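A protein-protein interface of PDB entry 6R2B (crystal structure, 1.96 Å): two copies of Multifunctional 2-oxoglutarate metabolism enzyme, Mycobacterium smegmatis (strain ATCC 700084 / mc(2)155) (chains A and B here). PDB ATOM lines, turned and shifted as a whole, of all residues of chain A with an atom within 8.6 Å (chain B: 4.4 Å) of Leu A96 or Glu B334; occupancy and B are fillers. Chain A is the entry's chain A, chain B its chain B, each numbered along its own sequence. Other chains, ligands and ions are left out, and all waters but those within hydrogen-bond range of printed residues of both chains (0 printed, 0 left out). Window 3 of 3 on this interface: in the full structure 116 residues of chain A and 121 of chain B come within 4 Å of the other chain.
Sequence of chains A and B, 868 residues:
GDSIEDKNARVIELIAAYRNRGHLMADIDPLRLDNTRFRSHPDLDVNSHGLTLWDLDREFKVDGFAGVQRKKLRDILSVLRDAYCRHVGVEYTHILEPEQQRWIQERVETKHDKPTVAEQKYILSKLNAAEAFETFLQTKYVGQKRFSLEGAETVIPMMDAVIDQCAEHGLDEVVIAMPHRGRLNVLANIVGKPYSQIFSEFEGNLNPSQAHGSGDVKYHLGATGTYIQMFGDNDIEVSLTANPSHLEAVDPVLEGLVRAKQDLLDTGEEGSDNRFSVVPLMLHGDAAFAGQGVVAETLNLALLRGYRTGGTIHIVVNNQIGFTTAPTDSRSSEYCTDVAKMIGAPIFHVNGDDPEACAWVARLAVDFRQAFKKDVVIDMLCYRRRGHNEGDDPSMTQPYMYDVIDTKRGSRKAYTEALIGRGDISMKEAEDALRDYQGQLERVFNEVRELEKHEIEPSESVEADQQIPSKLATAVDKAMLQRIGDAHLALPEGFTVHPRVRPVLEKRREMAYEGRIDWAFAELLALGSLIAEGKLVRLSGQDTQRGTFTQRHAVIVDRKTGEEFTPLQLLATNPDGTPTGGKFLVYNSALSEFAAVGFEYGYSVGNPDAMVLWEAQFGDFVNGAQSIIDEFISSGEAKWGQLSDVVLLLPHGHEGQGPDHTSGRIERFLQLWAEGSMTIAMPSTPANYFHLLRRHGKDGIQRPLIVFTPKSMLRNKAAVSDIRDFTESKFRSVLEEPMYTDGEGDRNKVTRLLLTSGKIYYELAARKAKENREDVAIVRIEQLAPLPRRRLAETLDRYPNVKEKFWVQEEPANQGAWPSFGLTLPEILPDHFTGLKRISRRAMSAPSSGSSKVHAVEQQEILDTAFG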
ATOM      1  N   TYR A  92      -7.231 -13.871 -19.920  1.00  0.00           N
ATOM      2  CA  TYR A  92      -7.949 -15.127 -19.734  1.00  0.00           C
ATOM      3  C   TYR A  92      -9.464 -15.003 -19.890  1.00  0.00           C
ATOM      4  O   TYR A  92     -10.131 -16.030 -19.990  1.00  0.00           O
ATOM      5  CB  TYR A  92      -7.619 -15.707 -18.335  1.00  0.00           C
ATOM      6  CG  TYR A  92      -8.274 -14.984 -17.171  1.00  0.00           C
ATOM      7  CD1 TYR A  92      -7.781 -13.762 -16.717  1.00  0.00           C
ATOM      8  CD2 TYR A  92      -9.377 -15.525 -16.518  1.00  0.00           C
ATOM      9  CE1 TYR A  92      -8.385 -13.088 -15.654  1.00  0.00           C
ATOM     10  CE2 TYR A  92      -9.981 -14.868 -15.446  1.00  0.00           C
ATOM     11  CZ  TYR A  92      -9.478 -13.650 -15.012  1.00  0.00           C
ATOM     12  OH  TYR A  92     -10.067 -12.996 -13.950  1.00  0.00           O
ATOM     13  N   THR A  93     -10.027 -13.787 -19.868  1.00  0.00           N
ATOM     14  CA  THR A  93     -11.493 -13.658 -19.926  1.00  0.00           C
ATOM     15  C   THR A  93     -12.058 -13.950 -21.332  1.00  0.00           C
ATOM     16  O   THR A  93     -13.276 -14.007 -21.488  1.00  0.00           O
ATOM     17  CB  THR A  93     -11.978 -12.308 -19.388  1.00  0.00           C
ATOM     18  OG1 THR A  93     -11.429 -11.263 -20.191  1.00  0.00           O
ATOM     19  CG2 THR A  93     -11.650 -12.119 -17.915  1.00  0.00           C
ATOM     20  N   HIS A  94     -11.181 -14.197 -22.325  1.00  0.00           N
ATOM     21  CA  HIS A  94     -11.577 -14.612 -23.675  1.00  0.00           C
ATOM     22  C   HIS A  94     -11.893 -16.114 -23.686  1.00  0.00           C
ATOM     23  O   HIS A  94     -12.484 -16.602 -24.646  1.00  0.00           O
ATOM     24  CB  HIS A  94     -10.453 -14.290 -24.691  1.00  0.00           C
ATOM     25  CG  HIS A  94      -9.164 -15.001 -24.407  1.00  0.00           C
ATOM     26  ND1 HIS A  94      -8.275 -14.525 -23.458  1.00  0.00           N
ATOM     27  CD2 HIS A  94      -8.665 -16.137 -24.946  1.00  0.00           C
ATOM     28  CE1 HIS A  94      -7.279 -15.393 -23.435  1.00  0.00           C
ATOM     29  NE2 HIS A  94      -7.462 -16.372 -24.321  1.00  0.00           N
ATOM     30  N   ILE A  95     -11.462 -16.856 -22.638  1.00  0.00           N
ATOM     31  CA  ILE A  95     -11.672 -18.307 -22.518  1.00  0.00           C
ATOM     32  C   ILE A  95     -13.177 -18.590 -22.339  1.00  0.00           C
ATOM     33  O   ILE A  95     -13.818 -18.024 -21.458  1.00  0.00           O
ATOM     34  CB  ILE A  95     -10.810 -18.909 -21.372  1.00  0.00           C
ATOM     35  CG1 ILE A  95      -9.292 -18.683 -21.645  1.00  0.00           C
ATOM     36  CG2 ILE A  95     -11.133 -20.401 -21.173  1.00  0.00           C
ATOM     37  CD1 ILE A  95      -8.375 -18.921 -20.474  1.00  0.00           C
ATOM     38  N   LEU A  96     -13.733 -19.475 -23.176  1.00  0.00           N
ATOM     39  CA  LEU A  96     -15.172 -19.752 -23.125  1.00  0.00           C
ATOM     40  C   LEU A  96     -15.577 -20.651 -21.950  1.00  0.00           C
ATOM     41  O   LEU A  96     -16.698 -20.516 -21.469  1.00  0.00           O
ATOM     42  CB  LEU A  96     -15.645 -20.368 -24.452  1.00  0.00           C
ATOM     43  CG  LEU A  96     -15.453 -19.494 -25.700  1.00  0.00           C
ATOM     44  CD1 LEU A  96     -15.892 -20.225 -26.927  1.00  0.00           C
ATOM     45  CD2 LEU A  96     -16.197 -18.139 -25.586  1.00  0.00           C
ATOM     46  N   GLU A  97     -14.691 -21.554 -21.490  1.00  0.00           N
ATOM     47  CA  GLU A  97     -14.983 -22.462 -20.372  1.00  0.00           C
ATOM     48  C   GLU A  97     -14.965 -21.672 -19.038  1.00  0.00           C
ATOM     49  O   GLU A  97     -13.910 -21.159 -18.661  1.00  0.00           O
ATOM     50  CB  GLU A  97     -13.979 -23.635 -20.333  1.00  0.00           C
ATOM     51  CG  GLU A  97     -13.962 -24.547 -21.557  1.00  0.00           C
ATOM     52  CD  GLU A  97     -13.336 -24.042 -22.848  1.00  0.00           C
ATOM     53  OE1 GLU A  97     -12.677 -22.975 -22.848  1.00  0.00           O
ATOM     54  OE2 GLU A  97     -13.517 -24.732 -23.878  1.00  0.00           O
ATOM     55  N   PRO A  98     -16.111 -21.535 -18.318  1.00  0.00           N
ATOM     56  CA  PRO A  98     -16.107 -20.741 -17.073  1.00  0.00           C
ATOM     57  C   PRO A  98     -15.237 -21.326 -15.964  1.00  0.00           C
ATOM     58  O   PRO A  98     -14.723 -20.561 -15.150  1.00  0.00           O
ATOM     59  CB  PRO A  98     -17.582 -20.739 -16.640  1.00  0.00           C
ATOM     60  CG  PRO A  98     -18.344 -21.095 -17.853  1.00  0.00           C
ATOM     61  CD  PRO A  98     -17.467 -22.041 -18.611  1.00  0.00           C
ATOM     62  N   GLU A  99     -15.084 -22.667 -15.918  1.00  0.00           N
ATOM     63  CA  GLU A  99     -14.284 -23.333 -14.884  1.00  0.00           C
ATOM     64  C   GLU A  99     -12.794 -22.997 -15.052  1.00  0.00           C
ATOM     65  O   GLU A  99     -12.089 -22.944 -14.052  1.00  0.00           O
ATOM     66  CB  GLU A  99     -14.518 -24.867 -14.869  1.00  0.00           C
ATOM     67  CG  GLU A  99     -14.151 -25.618 -16.145  1.00  0.00           C
ATOM     68  CD  GLU A  99     -15.188 -25.703 -17.256  1.00  0.00           C
ATOM     69  OE1 GLU A  99     -16.142 -24.890 -17.276  1.00  0.00           O
ATOM     70  OE2 GLU A  99     -15.030 -26.590 -18.124  1.00  0.00           O
ATOM     71  N   GLN A 100     -12.339 -22.727 -16.300  1.00  0.00           N
ATOM     72  CA  GLN A 100     -10.950 -22.357 -16.604  1.00  0.00           C
ATOM     73  C   GLN A 100     -10.707 -20.927 -16.177  1.00  0.00           C
ATOM     74  O   GLN A 100      -9.667 -20.650 -15.595  1.00  0.00           O
ATOM     75  CB  GLN A 100     -10.619 -22.562 -18.071  1.00  0.00           C
ATOM     76  CG  GLN A 100     -10.623 -24.030 -18.473  1.00  0.00           C
ATOM     77  CD  GLN A 100     -10.331 -24.245 -19.931  1.00  0.00           C
ATOM     78  OE1 GLN A 100      -9.792 -23.381 -20.623  1.00  0.00           O
ATOM     79  NE2 GLN A 100     -10.672 -25.416 -20.425  1.00  0.00           N
ATOM     80  N   GLN A 101     -11.677 -20.023 -16.418  1.00  0.00           N
ATOM     81  CA  GLN A 101     -11.586 -18.629 -15.968  1.00  0.00           C
ATOM     82  C   GLN A 101     -11.544 -18.572 -14.440  1.00  0.00           C
ATOM     83  O   GLN A 101     -10.741 -17.827 -13.887  1.00  0.00           O
ATOM     84  CB  GLN A 101     -12.760 -17.788 -16.474  1.00  0.00           C
ATOM     85  CG  GLN A 101     -12.704 -17.439 -17.945  1.00  0.00           C
ATOM     86  CD  GLN A 101     -13.546 -16.227 -18.257  1.00  0.00           C
ATOM     87  OE1 GLN A 101     -13.651 -15.279 -17.467  1.00  0.00           O
ATOM     88  NE2 GLN A 101     -14.153 -16.219 -19.426  1.00  0.00           N
ATOM     89  N   LEU A 303      -6.451 -29.724 -29.629  1.00  0.00           N
ATOM     90  CA  LEU A 303      -7.493 -30.505 -28.948  1.00  0.00           C
ATOM     91  C   LEU A 303      -8.094 -31.591 -29.874  1.00  0.00           C
ATOM     92  O   LEU A 303      -9.104 -32.193 -29.527  1.00  0.00           O
ATOM     93  CB  LEU A 303      -8.608 -29.586 -28.394  1.00  0.00           C
ATOM     94  CG  LEU A 303      -8.192 -28.396 -27.508  1.00  0.00           C
ATOM     95  CD1 LEU A 303      -9.407 -27.580 -27.104  1.00  0.00           C
ATOM     96  CD2 LEU A 303      -7.475 -28.863 -26.241  1.00  0.00           C
ATOM     97  N   LYS A 341      -5.172 -17.015 -29.135  1.00  0.00           N
ATOM     98  CA  LYS A 341      -6.571 -16.790 -28.754  1.00  0.00           C
ATOM     99  C   LYS A 341      -7.523 -17.581 -29.678  1.00  0.00           C
ATOM    100  O   LYS A 341      -8.689 -17.778 -29.328  1.00  0.00           O
ATOM    101  CB  LYS A 341      -6.921 -15.300 -28.729  1.00  0.00           C
ATOM    102  CG  LYS A 341      -6.042 -14.547 -27.732  1.00  0.00           C
ATOM    103  CD  LYS A 341      -6.674 -13.328 -27.154  1.00  0.00           C
ATOM    104  CE  LYS A 341      -6.286 -12.094 -27.912  1.00  0.00           C
ATOM    105  NZ  LYS A 341      -5.807 -11.038 -26.987  1.00  0.00           N
ATOM    106  N   MET A 342      -7.004 -18.127 -30.780  1.00  0.00           N
ATOM    107  CA  MET A 342      -7.801 -18.942 -31.705  1.00  0.00           C
ATOM    108  C   MET A 342      -8.250 -20.250 -31.034  1.00  0.00           C
ATOM    109  O   MET A 342      -9.240 -20.828 -31.465  1.00  0.00           O
ATOM    110  CB  MET A 342      -7.051 -19.215 -33.025  1.00  0.00           C
ATOM    111  CG  MET A 342      -6.093 -20.396 -33.009  1.00  0.00           C
ATOM    112  SD  MET A 342      -5.414 -20.759 -34.655  1.00  0.00           S
ATOM    113  CE  MET A 342      -6.662 -21.794 -35.278  1.00  0.00           C
ATOM    114  N   ILE A 343      -7.538 -20.716 -29.993  1.00  0.00           N
ATOM    115  CA  ILE A 343      -7.915 -21.956 -29.300  1.00  0.00           C
ATOM    116  C   ILE A 343      -8.260 -21.665 -27.840  1.00  0.00           C
ATOM    117  O   ILE A 343      -8.361 -22.602 -27.040  1.00  0.00           O
ATOM    118  CB  ILE A 343      -6.831 -23.070 -29.422  1.00  0.00           C
ATOM    119  CG1 ILE A 343      -5.429 -22.577 -28.929  1.00  0.00           C
ATOM    120  CG2 ILE A 343      -6.804 -23.634 -30.873  1.00  0.00           C
ATOM    121  CD1 ILE A 343      -4.468 -23.673 -28.467  1.00  0.00           C
ATOM    122  N   GLY A 344      -8.455 -20.383 -27.514  1.00  0.00           N
ATOM    123  CA  GLY A 344      -8.815 -19.964 -26.154  1.00  0.00           C
ATOM    124  C   GLY A 344      -7.771 -20.298 -25.108  1.00  0.00           C
ATOM    125  O   GLY A 344      -8.108 -20.666 -23.984  1.00  0.00           O
ATOM    126  N   ALA A 345      -6.490 -20.211 -25.477  1.00  0.00           N
ATOM    127  CA  ALA A 345      -5.407 -20.484 -24.527  1.00  0.00           C
ATOM    128  C   ALA A 345      -5.228 -19.306 -23.569  1.00  0.00           C
ATOM    129  O   ALA A 345      -5.344 -18.160 -24.013  1.00  0.00           O
ATOM    130  CB  ALA A 345      -4.101 -20.737 -25.281  1.00  0.00           C
ATOM    131  N   LYS A 374      -4.731 -28.412 -22.067  1.00  0.00           N
ATOM    132  CA  LYS A 374      -4.810 -27.360 -23.070  1.00  0.00           C
ATOM    133  C   LYS A 374      -3.560 -26.475 -23.013  1.00  0.00           C
ATOM    134  O   LYS A 374      -2.928 -26.360 -21.946  1.00  0.00           O
ATOM    135  CB  LYS A 374      -6.091 -26.566 -22.789  1.00  0.00           C
ATOM    136  CG  LYS A 374      -6.384 -25.363 -23.659  1.00  0.00           C
ATOM    137  CD  LYS A 374      -7.532 -24.615 -22.992  1.00  0.00           C
ATOM    138  CE  LYS A 374      -8.227 -23.713 -23.953  1.00  0.00           C
ATOM    139  NZ  LYS A 374      -9.414 -23.057 -23.336  1.00  0.00           N
ATOM    140  N   ARG B  21     -21.086 -13.402 -23.674  1.00  0.00           N
ATOM    141  CA  ARG B  21     -21.381 -14.808 -23.944  1.00  0.00           C
ATOM    142  C   ARG B  21     -22.753 -15.135 -24.521  1.00  0.00           C
ATOM    143  O   ARG B  21     -23.037 -16.323 -24.733  1.00  0.00           O
ATOM    144  CB  ARG B  21     -21.231 -15.581 -22.628  1.00  0.00           C
ATOM    145  CG  ARG B  21     -19.793 -15.577 -22.123  1.00  0.00           C
ATOM    146  CD  ARG B  21     -19.743 -16.050 -20.698  1.00  0.00           C
ATOM    147  NE  ARG B  21     -18.400 -16.505 -20.346  1.00  0.00           N
ATOM    148  CZ  ARG B  21     -17.970 -17.756 -20.483  1.00  0.00           C
ATOM    149  NH1 ARG B  21     -18.776 -18.696 -20.964  1.00  0.00           N
ATOM    150  NH2 ARG B  21     -16.732 -18.079 -20.138  1.00  0.00           N
ATOM    151  N   HIS B  23     -23.784 -14.983 -27.460  1.00  0.00           N
ATOM    152  CA  HIS B  23     -23.521 -15.667 -28.729  1.00  0.00           C
ATOM    153  C   HIS B  23     -23.523 -17.197 -28.566  1.00  0.00           C
ATOM    154  O   HIS B  23     -23.880 -17.889 -29.508  1.00  0.00           O
ATOM    155  CB  HIS B  23     -22.185 -15.192 -29.355  1.00  0.00           C
ATOM    156  CG  HIS B  23     -20.971 -15.423 -28.509  1.00  0.00           C
ATOM    157  ND1 HIS B  23     -20.166 -16.539 -28.687  1.00  0.00           N
ATOM    158  CD2 HIS B  23     -20.418 -14.636 -27.555  1.00  0.00           C
ATOM    159  CE1 HIS B  23     -19.183 -16.418 -27.810  1.00  0.00           C
ATOM    160  NE2 HIS B  23     -19.290 -15.291 -27.107  1.00  0.00           N
ATOM    161  N   LEU B  24     -23.154 -17.715 -27.373  1.00  0.00           N
ATOM    162  CA  LEU B  24     -23.148 -19.157 -27.084  1.00  0.00           C
ATOM    163  C   LEU B  24     -24.572 -19.708 -26.943  1.00  0.00           C
ATOM    164  O   LEU B  24     -24.762 -20.920 -27.011  1.00  0.00           O
ATOM    165  CB  LEU B  24     -22.348 -19.468 -25.801  1.00  0.00           C
ATOM    166  CG  LEU B  24     -20.861 -19.163 -25.776  1.00  0.00           C
ATOM    167  CD1 LEU B  24     -20.322 -19.272 -24.364  1.00  0.00           C
ATOM    168  CD2 LEU B  24     -20.074 -20.097 -26.708  1.00  0.00           C
ATOM    169  N   ARG B 331     -11.044 -28.546 -36.262  1.00  0.00           N
ATOM    170  CA  ARG B 331     -10.566 -27.409 -35.464  1.00  0.00           C
ATOM    171  C   ARG B 331     -10.582 -27.708 -33.978  1.00  0.00           C
ATOM    172  O   ARG B 331     -11.266 -28.621 -33.532  1.00  0.00           O
ATOM    173  CB  ARG B 331     -11.388 -26.132 -35.769  1.00  0.00           C
ATOM    174  CG  ARG B 331     -12.859 -26.228 -35.382  1.00  0.00           C
ATOM    175  CD  ARG B 331     -13.527 -24.893 -35.529  1.00  0.00           C
ATOM    176  NE  ARG B 331     -14.900 -24.906 -35.017  1.00  0.00           N
ATOM    177  CZ  ARG B 331     -15.971 -25.116 -35.767  1.00  0.00           C
ATOM    178  NH1 ARG B 331     -15.848 -25.298 -37.076  1.00  0.00           N
ATOM    179  NH2 ARG B 331     -17.181 -25.099 -35.224  1.00  0.00           N
ATOM    180  N   SER B 333     -11.331 -25.317 -31.647  1.00  0.00           N
ATOM    181  CA  SER B 333     -12.041 -24.198 -31.045  1.00  0.00           C
ATOM    182  C   SER B 333     -13.513 -24.260 -31.351  1.00  0.00           C
ATOM    183  O   SER B 333     -13.930 -24.995 -32.238  1.00  0.00           O
ATOM    184  CB  SER B 333     -11.459 -22.886 -31.543  1.00  0.00           C
ATOM    185  OG  SER B 333     -11.752 -22.676 -32.911  1.00  0.00           O
ATOM    186  N   GLU B 334     -14.298 -23.479 -30.605  1.00  0.00           N
ATOM    187  CA  GLU B 334     -15.732 -23.407 -30.711  1.00  0.00           C
ATOM    188  C   GLU B 334     -16.185 -23.014 -32.101  1.00  0.00           C
ATOM    189  O   GLU B 334     -17.110 -23.636 -32.623  1.00  0.00           O
ATOM    190  CB  GLU B 334     -16.260 -22.401 -29.669  1.00  0.00           C
ATOM    191  CG  GLU B 334     -17.775 -22.240 -29.610  1.00  0.00           C
ATOM    192  CD  GLU B 334     -18.649 -23.466 -29.398  1.00  0.00           C
ATOM    193  OE1 GLU B 334     -18.178 -24.474 -28.820  1.00  0.00           O
ATOM    194  OE2 GLU B 334     -19.831 -23.402 -29.799  1.00  0.00           O
ATOM    195  N   TYR B 335     -15.542 -21.989 -32.703  1.00  0.00           N
ATOM    196  CA  TYR B 335     -15.938 -21.494 -34.015  1.00  0.00           C
ATOM    197  C   TYR B 335     -14.847 -21.633 -35.028  1.00  0.00           C
ATOM    198  O   TYR B 335     -13.665 -21.473 -34.679  1.00  0.00           O
ATOM    199  CB  TYR B 335     -16.327 -20.010 -33.923  1.00  0.00           C
ATOM    200  CG  TYR B 335     -17.445 -19.714 -32.950  1.00  0.00           C
ATOM    201  CD1 TYR B 335     -18.761 -20.049 -33.247  1.00  0.00           C
ATOM    202  CD2 TYR B 335     -17.195 -19.046 -31.753  1.00  0.00           C
ATOM    203  CE1 TYR B 335     -19.806 -19.724 -32.380  1.00  0.00           C
ATOM    204  CE2 TYR B 335     -18.226 -18.748 -30.861  1.00  0.00           C
ATOM    205  CZ  TYR B 335     -19.534 -19.067 -31.190  1.00  0.00           C
ATOM    206  OH  TYR B 335     -20.560 -18.735 -30.336  1.00  0.00           O
ATOM    207  N   ASP B 338     -12.448 -18.375 -35.147  1.00  0.00           N
ATOM    208  CA  ASP B 338     -11.686 -17.967 -33.962  1.00  0.00           C
ATOM    209  C   ASP B 338     -10.270 -17.463 -34.279  1.00  0.00           C
ATOM    210  O   ASP B 338      -9.737 -16.680 -33.487  1.00  0.00           O
ATOM    211  CB  ASP B 338     -11.650 -19.081 -32.908  1.00  0.00           C
ATOM    212  CG  ASP B 338     -12.950 -19.214 -32.099  1.00  0.00           C
ATOM    213  OD1 ASP B 338     -13.659 -18.203 -31.933  1.00  0.00           O
ATOM    214  OD2 ASP B 338     -13.239 -20.324 -31.623  1.00  0.00           O
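The backbone carbonyl oxygen of Ile A95 sits at hydrogen-bond distance from the guanidinium group of Arg B21 (3.2 Å). O of Leu A96 is in hydrogen-bond range of NH2 of Arg B21 (2.8 Å). NH2 of Arg B21 sits close to NE2 of Gln A101, at 3.3 Å. The backbone carbonyl oxygen (O) of Met A342 sits close to the side-chain hydroxyl (OG) of Ser B333 (3.4 Å).
The side-chain amide nitrogen (NE2) of Gln A101 is in hydrogen-bond range of the backbone carbonyl oxygen (O) of Thr A93, at 3.1 Å. The backbone carbonyl oxygen (O) of Ile A95 sits at hydrogen-bond distance from the side-chain amide nitrogen (NE2) of Gln A101 (2.7 Å). The backbone carbonyl oxygen (O) of Ser B333 is in hydrogen-bond range of the guanidinium group (NE) of Arg B331 (2.9 Å). OD2 of Asp B338 is in hydrogen-bond range of OG of Ser B333, 3.1 Å away. The side-chain carboxylate (OD2) of Asp B338 sits at hydrogen-bond distance from the backbone NH (N) of Glu B334. The side-chain carboxylate (OD2) of Asp B338 is in hydrogen-bond range of the backbone NH (N) of Tyr B335 (3.0 Å).
Leu A96 touches Glu B334. Pro A98 touches Arg B21 (CG to NH1, 3.95 Å). Met A342 touches Asp B338.
Of the printed residues of chain B, Pro A98 touches Arg B21 (3.95 Å). Printed residues of chain B within 4 Å of Gln A101: Arg B21 (3.3 Å). Ile A343 touches none of the printed residues of chain B. Of the printed residues of chain A, Arg B21 touches Ile A95 (3.2 Å), Leu A96 (2.8 Å), Pro A98 (3.95 Å) and Gln A101 (3.3 Å). Leu B24 touches none of the printed residues of chain A. Ser B333 touches just one residue of chain A: Met A342. Glu B334 touches one residue of chain A. Tyr B335 touches none of the printed residues of chain A. Of the printed residues of chain A, Asp B338 touches Met A342. The nearest residue of chain A that does not touch Glu B334 is Met A342 (5.8 Å).
Printed residues of chain A that touch a printed residue of chain B: Ile A95, Leu A96, Pro A98, Gln A101 and Met A342. Hydrophobic or aromatic side chains of chain A within 4 Å of the printed part of chain B: Leu A96, Pro A98 and Met A342. Of the 8 printed residues of chain B, 4 touch a printed residue of chain A. Printed residues of chain B that touch a printed residue of chain A: Arg B21, Ser B333, Glu B334 and Asp B338. Among the printed residues, no Asp or Glu carboxylate lies within 4 Å of a Lys or Arg side-chain nitrogen of the other chain.
No position is printed for both chains. Of the 7 pairs that touch across the chains among the printed residues, none has its exchanged pair printed and touching as well.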
